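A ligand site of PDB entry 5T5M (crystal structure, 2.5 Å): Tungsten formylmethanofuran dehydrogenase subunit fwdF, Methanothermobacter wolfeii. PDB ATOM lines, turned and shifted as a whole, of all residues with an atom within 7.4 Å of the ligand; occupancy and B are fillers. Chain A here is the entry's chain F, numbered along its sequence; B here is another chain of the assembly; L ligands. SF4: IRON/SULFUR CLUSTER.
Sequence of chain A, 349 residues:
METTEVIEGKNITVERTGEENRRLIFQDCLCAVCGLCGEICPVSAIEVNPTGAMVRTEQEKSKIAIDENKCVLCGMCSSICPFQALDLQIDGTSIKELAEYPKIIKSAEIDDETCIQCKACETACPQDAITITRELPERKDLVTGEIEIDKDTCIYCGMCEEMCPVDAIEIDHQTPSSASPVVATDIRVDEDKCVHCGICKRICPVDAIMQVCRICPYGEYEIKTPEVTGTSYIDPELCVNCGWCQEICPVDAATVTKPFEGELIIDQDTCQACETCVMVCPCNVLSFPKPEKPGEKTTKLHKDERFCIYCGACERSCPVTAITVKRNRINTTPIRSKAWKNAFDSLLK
The side-chain sulfur (SG) of Cys 154 is bound to an iron atom (FE3) of the ligand. The side-chain sulfur (SG) of Cys 204 is bound to an iron atom (FE1) of the ligand (2.4 Å). N of Cys 157 sits close to S1 of the ligand (3.7 Å). An iron atom (FE2) of the ligand is bound by the side-chain sulfur of Cys 157. The side-chain sulfur of Cys 160 is bound to an iron atom (FE4) of the ligand (2.6 Å). S1 of the ligand lies close to N of Gly 158, 3.6 Å away.
The backbone NH (N) of Tyr 156 sits close to the side-chain sulfur (SG) of Cys 154 (3.4 Å). The side-chain sulfur (SG) of Cys 204 sits close to the backbone NH (N) of Val 206, at 3.3 Å. The backbone NH of Ala 208 sits close to the side-chain sulfur of Cys 204 (3.2 Å). SG of Cys 204 sits close to N of Asp 207, at 3.2 Å. The side-chain sulfur of Cys 157 lies close to the backbone NH of Met 159, 3.5 Å away. The backbone carbonyl oxygen (O) of Cys 157 is in hydrogen-bond range of the guanidinium group (NH1) of Arg 134 of chain B (3.0 Å).
N of Ile 155 touches S4 of the ligand, at 3.8 Å. N of Tyr 156 touches FE3 of the ligand (3.6 Å). Pro 205 touches the ligand. CD1 of Ile 209 touches S2 of the ligand, at 3.8 Å. Hydrophobic or aromatic side chains within 4 Å of the ligand: Pro 205 and Ile 209. The nearest printed residue that does not touch the ligand is Ile 187 (4.04 Å).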
ATOM      1  N   ILE A 149       0.458  -3.903  13.790  1.00  0.00           N
ATOM      2  CA  ILE A 149       0.469  -2.970  14.903  1.00  0.00           C
ATOM      3  C   ILE A 149       1.926  -2.729  15.266  1.00  0.00           C
ATOM      4  O   ILE A 149       2.680  -3.677  15.501  1.00  0.00           O
ATOM      5  CB  ILE A 149      -0.317  -3.535  16.105  1.00  0.00           C
ATOM      6  CG1 ILE A 149      -1.773  -3.733  15.697  1.00  0.00           C
ATOM      7  CG2 ILE A 149      -0.201  -2.590  17.283  1.00  0.00           C
ATOM      8  CD1 ILE A 149      -2.685  -4.157  16.831  1.00  0.00           C
ATOM      9  N   ASP A 150       2.318  -1.457  15.294  1.00  0.00           N
ATOM     10  CA  ASP A 150       3.655  -1.036  15.758  1.00  0.00           C
ATOM     11  C   ASP A 150       3.637  -1.090  17.279  1.00  0.00           C
ATOM     12  O   ASP A 150       3.122  -0.189  17.950  1.00  0.00           O
ATOM     13  CB  ASP A 150       3.971   0.364  15.240  1.00  0.00           C
ATOM     14  CG  ASP A 150       5.383   0.827  15.593  1.00  0.00           C
ATOM     15  OD1 ASP A 150       6.004   0.328  16.549  1.00  0.00           O
ATOM     16  OD2 ASP A 150       5.865   1.740  14.886  1.00  0.00           O
ATOM     17  N   LYS A 151       4.236  -2.150  17.846  1.00  0.00           N
ATOM     18  CA  LYS A 151       4.160  -2.327  19.300  1.00  0.00           C
ATOM     19  C   LYS A 151       5.004  -1.320  20.061  1.00  0.00           C
ATOM     20  O   LYS A 151       4.834  -1.212  21.285  1.00  0.00           O
ATOM     21  CB  LYS A 151       4.573  -3.754  19.669  1.00  0.00           C
ATOM     22  CG  LYS A 151       3.733  -4.835  18.980  1.00  0.00           C
ATOM     23  CD  LYS A 151       4.060  -6.246  19.441  1.00  0.00           C
ATOM     24  CE  LYS A 151       3.348  -7.293  18.555  1.00  0.00           C
ATOM     25  NZ  LYS A 151       3.507  -8.724  18.972  1.00  0.00           N
ATOM     26  N   THR A 153       5.087   2.213  19.099  1.00  0.00           N
ATOM     27  CA  THR A 153       4.188   3.356  19.136  1.00  0.00           C
ATOM     28  C   THR A 153       2.987   3.104  20.050  1.00  0.00           C
ATOM     29  O   THR A 153       2.532   4.006  20.764  1.00  0.00           O
ATOM     30  CB  THR A 153       3.687   3.654  17.729  1.00  0.00           C
ATOM     31  OG1 THR A 153       4.794   3.644  16.826  1.00  0.00           O
ATOM     32  CG2 THR A 153       3.008   5.006  17.684  1.00  0.00           C
ATOM     33  N   CYS A 154       2.457   1.886  20.021  1.00  0.00           N
ATOM     34  CA  CYS A 154       1.312   1.526  20.828  1.00  0.00           C
ATOM     35  C   CYS A 154       1.535   1.899  22.292  1.00  0.00           C
ATOM     36  O   CYS A 154       2.565   1.592  22.878  1.00  0.00           O
ATOM     37  CB  CYS A 154       1.049   0.017  20.684  1.00  0.00           C
ATOM     38  SG  CYS A 154      -0.167  -0.772  21.799  1.00  0.00           S
ATOM     39  N   ILE A 155       0.541   2.586  22.868  1.00  0.00           N
ATOM     40  CA  ILE A 155       0.519   2.960  24.276  1.00  0.00           C
ATOM     41  C   ILE A 155      -0.464   2.113  25.081  1.00  0.00           C
ATOM     42  O   ILE A 155      -0.671   2.386  26.262  1.00  0.00           O
ATOM     43  CB  ILE A 155       0.186   4.465  24.439  1.00  0.00           C
ATOM     44  CG1 ILE A 155      -1.250   4.746  24.001  1.00  0.00           C
ATOM     45  CG2 ILE A 155       1.159   5.292  23.622  1.00  0.00           C
ATOM     46  CD1 ILE A 155      -1.671   6.200  24.079  1.00  0.00           C
ATOM     47  N   TYR A 156      -1.086   1.113  24.459  1.00  0.00           N
ATOM     48  CA  TYR A 156      -1.847   0.094  25.181  1.00  0.00           C
ATOM     49  C   TYR A 156      -3.102   0.661  25.846  1.00  0.00           C
ATOM     50  O   TYR A 156      -3.560   0.143  26.870  1.00  0.00           O
ATOM     51  CB  TYR A 156      -0.951  -0.634  26.194  1.00  0.00           C
ATOM     52  CG  TYR A 156       0.143  -1.407  25.510  1.00  0.00           C
ATOM     53  CD1 TYR A 156      -0.143  -2.609  24.861  1.00  0.00           C
ATOM     54  CD2 TYR A 156       1.448  -0.934  25.463  1.00  0.00           C
ATOM     55  CE1 TYR A 156       0.851  -3.329  24.214  1.00  0.00           C
ATOM     56  CE2 TYR A 156       2.450  -1.651  24.822  1.00  0.00           C
ATOM     57  CZ  TYR A 156       2.145  -2.840  24.192  1.00  0.00           C
ATOM     58  OH  TYR A 156       3.117  -3.562  23.540  1.00  0.00           O
ATOM     59  N   CYS A 157      -3.684   1.699  25.248  1.00  0.00           N
ATOM     60  CA  CYS A 157      -4.934   2.264  25.763  1.00  0.00           C
ATOM     61  C   CYS A 157      -6.064   1.253  25.728  1.00  0.00           C
ATOM     62  O   CYS A 157      -7.024   1.411  26.486  1.00  0.00           O
ATOM     63  CB  CYS A 157      -5.309   3.514  24.955  1.00  0.00           C
ATOM     64  SG  CYS A 157      -5.993   3.217  23.258  1.00  0.00           S
ATOM     65  N   GLY A 158      -5.990   0.240  24.867  1.00  0.00           N
ATOM     66  CA  GLY A 158      -6.986  -0.805  24.864  1.00  0.00           C
ATOM     67  C   GLY A 158      -8.253  -0.493  24.101  1.00  0.00           C
ATOM     68  O   GLY A 158      -9.219  -1.259  24.202  1.00  0.00           O
ATOM     69  N   MET A 159      -8.292   0.597  23.332  1.00  0.00           N
ATOM     70  CA  MET A 159      -9.505   0.992  22.627  1.00  0.00           C
ATOM     71  C   MET A 159      -9.767   0.106  21.418  1.00  0.00           C
ATOM     72  O   MET A 159     -10.916  -0.257  21.149  1.00  0.00           O
ATOM     73  CB  MET A 159      -9.418   2.466  22.222  1.00  0.00           C
ATOM     74  CG  MET A 159      -9.457   3.424  23.427  1.00  0.00           C
ATOM     75  SD  MET A 159      -9.728   5.168  23.042  1.00  0.00           S
ATOM     76  CE  MET A 159      -8.448   5.454  21.836  1.00  0.00           C
ATOM     77  N   CYS A 160      -8.738  -0.230  20.648  1.00  0.00           N
ATOM     78  CA  CYS A 160      -8.893  -1.184  19.547  1.00  0.00           C
ATOM     79  C   CYS A 160      -9.472  -2.502  20.060  1.00  0.00           C
ATOM     80  O   CYS A 160     -10.396  -3.065  19.445  1.00  0.00           O
ATOM     81  CB  CYS A 160      -7.553  -1.438  18.874  1.00  0.00           C
ATOM     82  SG  CYS A 160      -6.391  -2.388  19.915  1.00  0.00           S
ATOM     83  N   GLU A 161      -8.942  -3.007  21.166  1.00  0.00           N
ATOM     84  CA  GLU A 161      -9.368  -4.295  21.701  1.00  0.00           C
ATOM     85  C   GLU A 161     -10.860  -4.268  22.047  1.00  0.00           C
ATOM     86  O   GLU A 161     -11.588  -5.222  21.745  1.00  0.00           O
ATOM     87  CB  GLU A 161      -8.519  -4.646  22.925  1.00  0.00           C
ATOM     88  CG  GLU A 161      -8.757  -6.024  23.539  1.00  0.00           C
ATOM     89  CD  GLU A 161      -7.897  -6.271  24.796  1.00  0.00           C
ATOM     90  OE1 GLU A 161      -7.355  -7.390  24.952  1.00  0.00           O
ATOM     91  OE2 GLU A 161      -7.760  -5.337  25.625  1.00  0.00           O
ATOM     92  N   ILE A 169      -8.263  -8.640  18.291  1.00  0.00           N
ATOM     93  CA  ILE A 169      -7.105  -8.035  18.954  1.00  0.00           C
ATOM     94  C   ILE A 169      -7.084  -8.479  20.407  1.00  0.00           C
ATOM     95  O   ILE A 169      -8.101  -8.383  21.119  1.00  0.00           O
ATOM     96  CB  ILE A 169      -7.137  -6.498  18.859  1.00  0.00           C
ATOM     97  CG1 ILE A 169      -7.016  -6.050  17.404  1.00  0.00           C
ATOM     98  CG2 ILE A 169      -5.988  -5.914  19.654  1.00  0.00           C
ATOM     99  CD1 ILE A 169      -7.332  -4.596  17.193  1.00  0.00           C
ATOM    100  N   ILE A 171      -4.657  -8.045  24.028  1.00  0.00           N
ATOM    101  CA  ILE A 171      -3.607  -7.321  24.736  1.00  0.00           C
ATOM    102  C   ILE A 171      -3.277  -8.094  26.002  1.00  0.00           C
ATOM    103  O   ILE A 171      -4.182  -8.570  26.704  1.00  0.00           O
ATOM    104  CB  ILE A 171      -4.035  -5.881  25.069  1.00  0.00           C
ATOM    105  CG1 ILE A 171      -4.251  -5.084  23.774  1.00  0.00           C
ATOM    106  CG2 ILE A 171      -2.999  -5.192  25.961  1.00  0.00           C
ATOM    107  CD1 ILE A 171      -4.871  -3.724  24.004  1.00  0.00           C
ATOM    108  N   ILE A 187       0.637  -7.018  22.229  1.00  0.00           N
ATOM    109  CA  ILE A 187      -0.617  -6.837  21.522  1.00  0.00           C
ATOM    110  C   ILE A 187      -0.564  -7.657  20.237  1.00  0.00           C
ATOM    111  O   ILE A 187       0.468  -7.703  19.567  1.00  0.00           O
ATOM    112  CB  ILE A 187      -0.897  -5.347  21.259  1.00  0.00           C
ATOM    113  CG1 ILE A 187      -2.211  -5.158  20.486  1.00  0.00           C
ATOM    114  CG2 ILE A 187       0.269  -4.718  20.521  1.00  0.00           C
ATOM    115  CD1 ILE A 187      -2.696  -3.718  20.463  1.00  0.00           C
ATOM    116  N   CYS A 200     -10.144  -0.353  14.107  1.00  0.00           N
ATOM    117  CA  CYS A 200      -8.992  -0.213  15.008  1.00  0.00           C
ATOM    118  C   CYS A 200      -8.120   0.976  14.595  1.00  0.00           C
ATOM    119  O   CYS A 200      -7.853   1.870  15.393  1.00  0.00           O
ATOM    120  CB  CYS A 200      -8.184  -1.509  15.003  1.00  0.00           C
ATOM    121  SG  CYS A 200      -7.641  -2.031  13.353  1.00  0.00           S
ATOM    122  N   LYS A 201      -7.679   0.980  13.345  1.00  0.00           N
ATOM    123  CA  LYS A 201      -6.845   2.050  12.819  1.00  0.00           C
ATOM    124  C   LYS A 201      -7.469   3.421  13.084  1.00  0.00           C
ATOM    125  O   LYS A 201      -6.760   4.363  13.438  1.00  0.00           O
ATOM    126  CB  LYS A 201      -6.652   1.824  11.322  1.00  0.00           C
ATOM    127  CG  LYS A 201      -6.277   3.039  10.503  1.00  0.00           C
ATOM    128  CD  LYS A 201      -6.193   2.692   9.012  1.00  0.00           C
ATOM    129  CE  LYS A 201      -7.560   2.328   8.430  1.00  0.00           C
ATOM    130  NZ  LYS A 201      -7.470   1.829   7.036  1.00  0.00           N
ATOM    131  N   ILE A 203      -9.651   4.331  15.423  1.00  0.00           N
ATOM    132  CA  ILE A 203      -9.787   4.716  16.819  1.00  0.00           C
ATOM    133  C   ILE A 203      -8.441   4.946  17.489  1.00  0.00           C
ATOM    134  O   ILE A 203      -8.387   5.607  18.535  1.00  0.00           O
ATOM    135  CB  ILE A 203     -10.598   3.662  17.594  1.00  0.00           C
ATOM    136  CG1 ILE A 203     -11.056   4.197  18.957  1.00  0.00           C
ATOM    137  CG2 ILE A 203      -9.781   2.401  17.811  1.00  0.00           C
ATOM    138  CD1 ILE A 203     -11.863   5.467  18.902  1.00  0.00           C
ATOM    139  N   CYS A 204      -7.354   4.428  16.921  1.00  0.00           N
ATOM    140  CA  CYS A 204      -6.073   4.479  17.603  1.00  0.00           C
ATOM    141  C   CYS A 204      -5.661   5.924  17.846  1.00  0.00           C
ATOM    142  O   CYS A 204      -5.628   6.732  16.904  1.00  0.00           O
ATOM    143  CB  CYS A 204      -5.002   3.783  16.779  1.00  0.00           C
ATOM    144  SG  CYS A 204      -3.342   4.017  17.461  1.00  0.00           S
ATOM    145  N   PRO A 205      -5.315   6.300  19.084  1.00  0.00           N
ATOM    146  CA  PRO A 205      -4.934   7.690  19.349  1.00  0.00           C
ATOM    147  C   PRO A 205      -3.509   8.048  18.966  1.00  0.00           C
ATOM    148  O   PRO A 205      -3.183   9.237  18.970  1.00  0.00           O
ATOM    149  CB  PRO A 205      -5.137   7.810  20.864  1.00  0.00           C
ATOM    150  CG  PRO A 205      -4.812   6.434  21.361  1.00  0.00           C
ATOM    151  CD  PRO A 205      -5.291   5.476  20.300  1.00  0.00           C
ATOM    152  N   VAL A 206      -2.663   7.074  18.616  1.00  0.00           N
ATOM    153  CA  VAL A 206      -1.265   7.338  18.289  1.00  0.00           C
ATOM    154  C   VAL A 206      -0.886   6.798  16.912  1.00  0.00           C
ATOM    155  O   VAL A 206       0.288   6.675  16.614  1.00  0.00           O
ATOM    156  CB  VAL A 206      -0.337   6.760  19.371  1.00  0.00           C
ATOM    157  CG1 VAL A 206      -0.662   7.373  20.719  1.00  0.00           C
ATOM    158  CG2 VAL A 206      -0.441   5.241  19.427  1.00  0.00           C
ATOM    159  N   ASP A 207      -1.872   6.472  16.087  1.00  0.00           N
ATOM    160  CA  ASP A 207      -1.648   5.929  14.747  1.00  0.00           C
ATOM    161  C   ASP A 207      -0.587   4.827  14.750  1.00  0.00           C
ATOM    162  O   ASP A 207       0.356   4.818  13.965  1.00  0.00           O
ATOM    163  CB  ASP A 207      -1.255   7.046  13.778  1.00  0.00           C
ATOM    164  CG  ASP A 207      -2.360   8.069  13.611  1.00  0.00           C
ATOM    165  OD1 ASP A 207      -3.549   7.677  13.702  1.00  0.00           O
ATOM    166  OD2 ASP A 207      -2.047   9.252  13.384  1.00  0.00           O
ATOM    167  N   ALA A 208      -0.780   3.847  15.635  1.00  0.00           N
ATOM    168  CA  ALA A 208       0.104   2.704  15.726  1.00  0.00           C
ATOM    169  C   ALA A 208      -0.285   1.542  14.818  1.00  0.00           C
ATOM    170  O   ALA A 208       0.475   0.575  14.710  1.00  0.00           O
ATOM    171  CB  ALA A 208       0.161   2.182  17.174  1.00  0.00           C
ATOM    172  N   ILE A 209      -1.454   1.611  14.165  1.00  0.00           N
ATOM    173  CA  ILE A 209      -1.988   0.481  13.422  1.00  0.00           C
ATOM    174  C   ILE A 209      -2.046   0.847  11.955  1.00  0.00           C
ATOM    175  O   ILE A 209      -2.713   1.814  11.572  1.00  0.00           O
ATOM    176  CB  ILE A 209      -3.383   0.075  13.917  1.00  0.00           C
ATOM    177  CG1 ILE A 209      -3.352  -0.212  15.412  1.00  0.00           C
ATOM    178  CG2 ILE A 209      -3.898  -1.129  13.118  1.00  0.00           C
ATOM    179  CD1 ILE A 209      -4.686  -0.705  15.980  1.00  0.00           C
ATOM    180  N   CYS B 118      -6.146   7.126  28.212  1.00  0.00           N
ATOM    181  CA  CYS B 118      -5.531   5.848  27.906  1.00  0.00           C
ATOM    182  C   CYS B 118      -5.677   4.841  29.047  1.00  0.00           C
ATOM    183  O   CYS B 118      -5.564   3.638  28.800  1.00  0.00           O
ATOM    184  CB  CYS B 118      -4.048   6.043  27.554  1.00  0.00           C
ATOM    185  SG  CYS B 118      -2.848   5.928  28.950  1.00  0.00           S
ATOM    186  N   ARG B 134     -14.184   7.107  30.074  1.00  0.00           N
ATOM    187  CA  ARG B 134     -14.063   7.519  28.675  1.00  0.00           C
ATOM    188  C   ARG B 134     -15.254   7.035  27.864  1.00  0.00           C
ATOM    189  O   ARG B 134     -15.779   5.949  28.096  1.00  0.00           O
ATOM    190  CB  ARG B 134     -12.756   7.019  28.062  1.00  0.00           C
ATOM    191  CG  ARG B 134     -12.691   5.540  27.770  1.00  0.00           C
ATOM    192  CD  ARG B 134     -11.327   5.164  27.206  1.00  0.00           C
ATOM    193  NE  ARG B 134     -11.211   3.735  26.994  1.00  0.00           N
ATOM    194  CZ  ARG B 134     -10.051   3.082  26.909  1.00  0.00           C
ATOM    195  NH1 ARG B 134     -10.030   1.772  26.707  1.00  0.00           N
ATOM    196  NH2 ARG B 134      -8.916   3.761  27.037  1.00  0.00           N
HETATM  197 FE1  SF4 L   1      -3.652   2.230  19.078  1.00  0.00          FE
HETATM  198 FE2  SF4 L   1      -4.477   1.763  21.942  1.00  0.00          FE
HETATM  199 FE3  SF4 L   1      -2.172   0.371  21.136  1.00  0.00          FE
HETATM  200 FE4  SF4 L   1      -4.881  -0.340  20.128  1.00  0.00          FE
HETATM  201  S1  SF4 L   1      -3.897  -0.152  22.013  1.00  0.00           S
HETATM  202  S2  SF4 L   1      -3.100   0.307  19.301  1.00  0.00           S
HETATM  203  S3  SF4 L   1      -5.329   1.577  19.998  1.00  0.00           S
HETATM  204  S4  SF4 L   1      -2.720   2.256  20.929  1.00  0.00           S
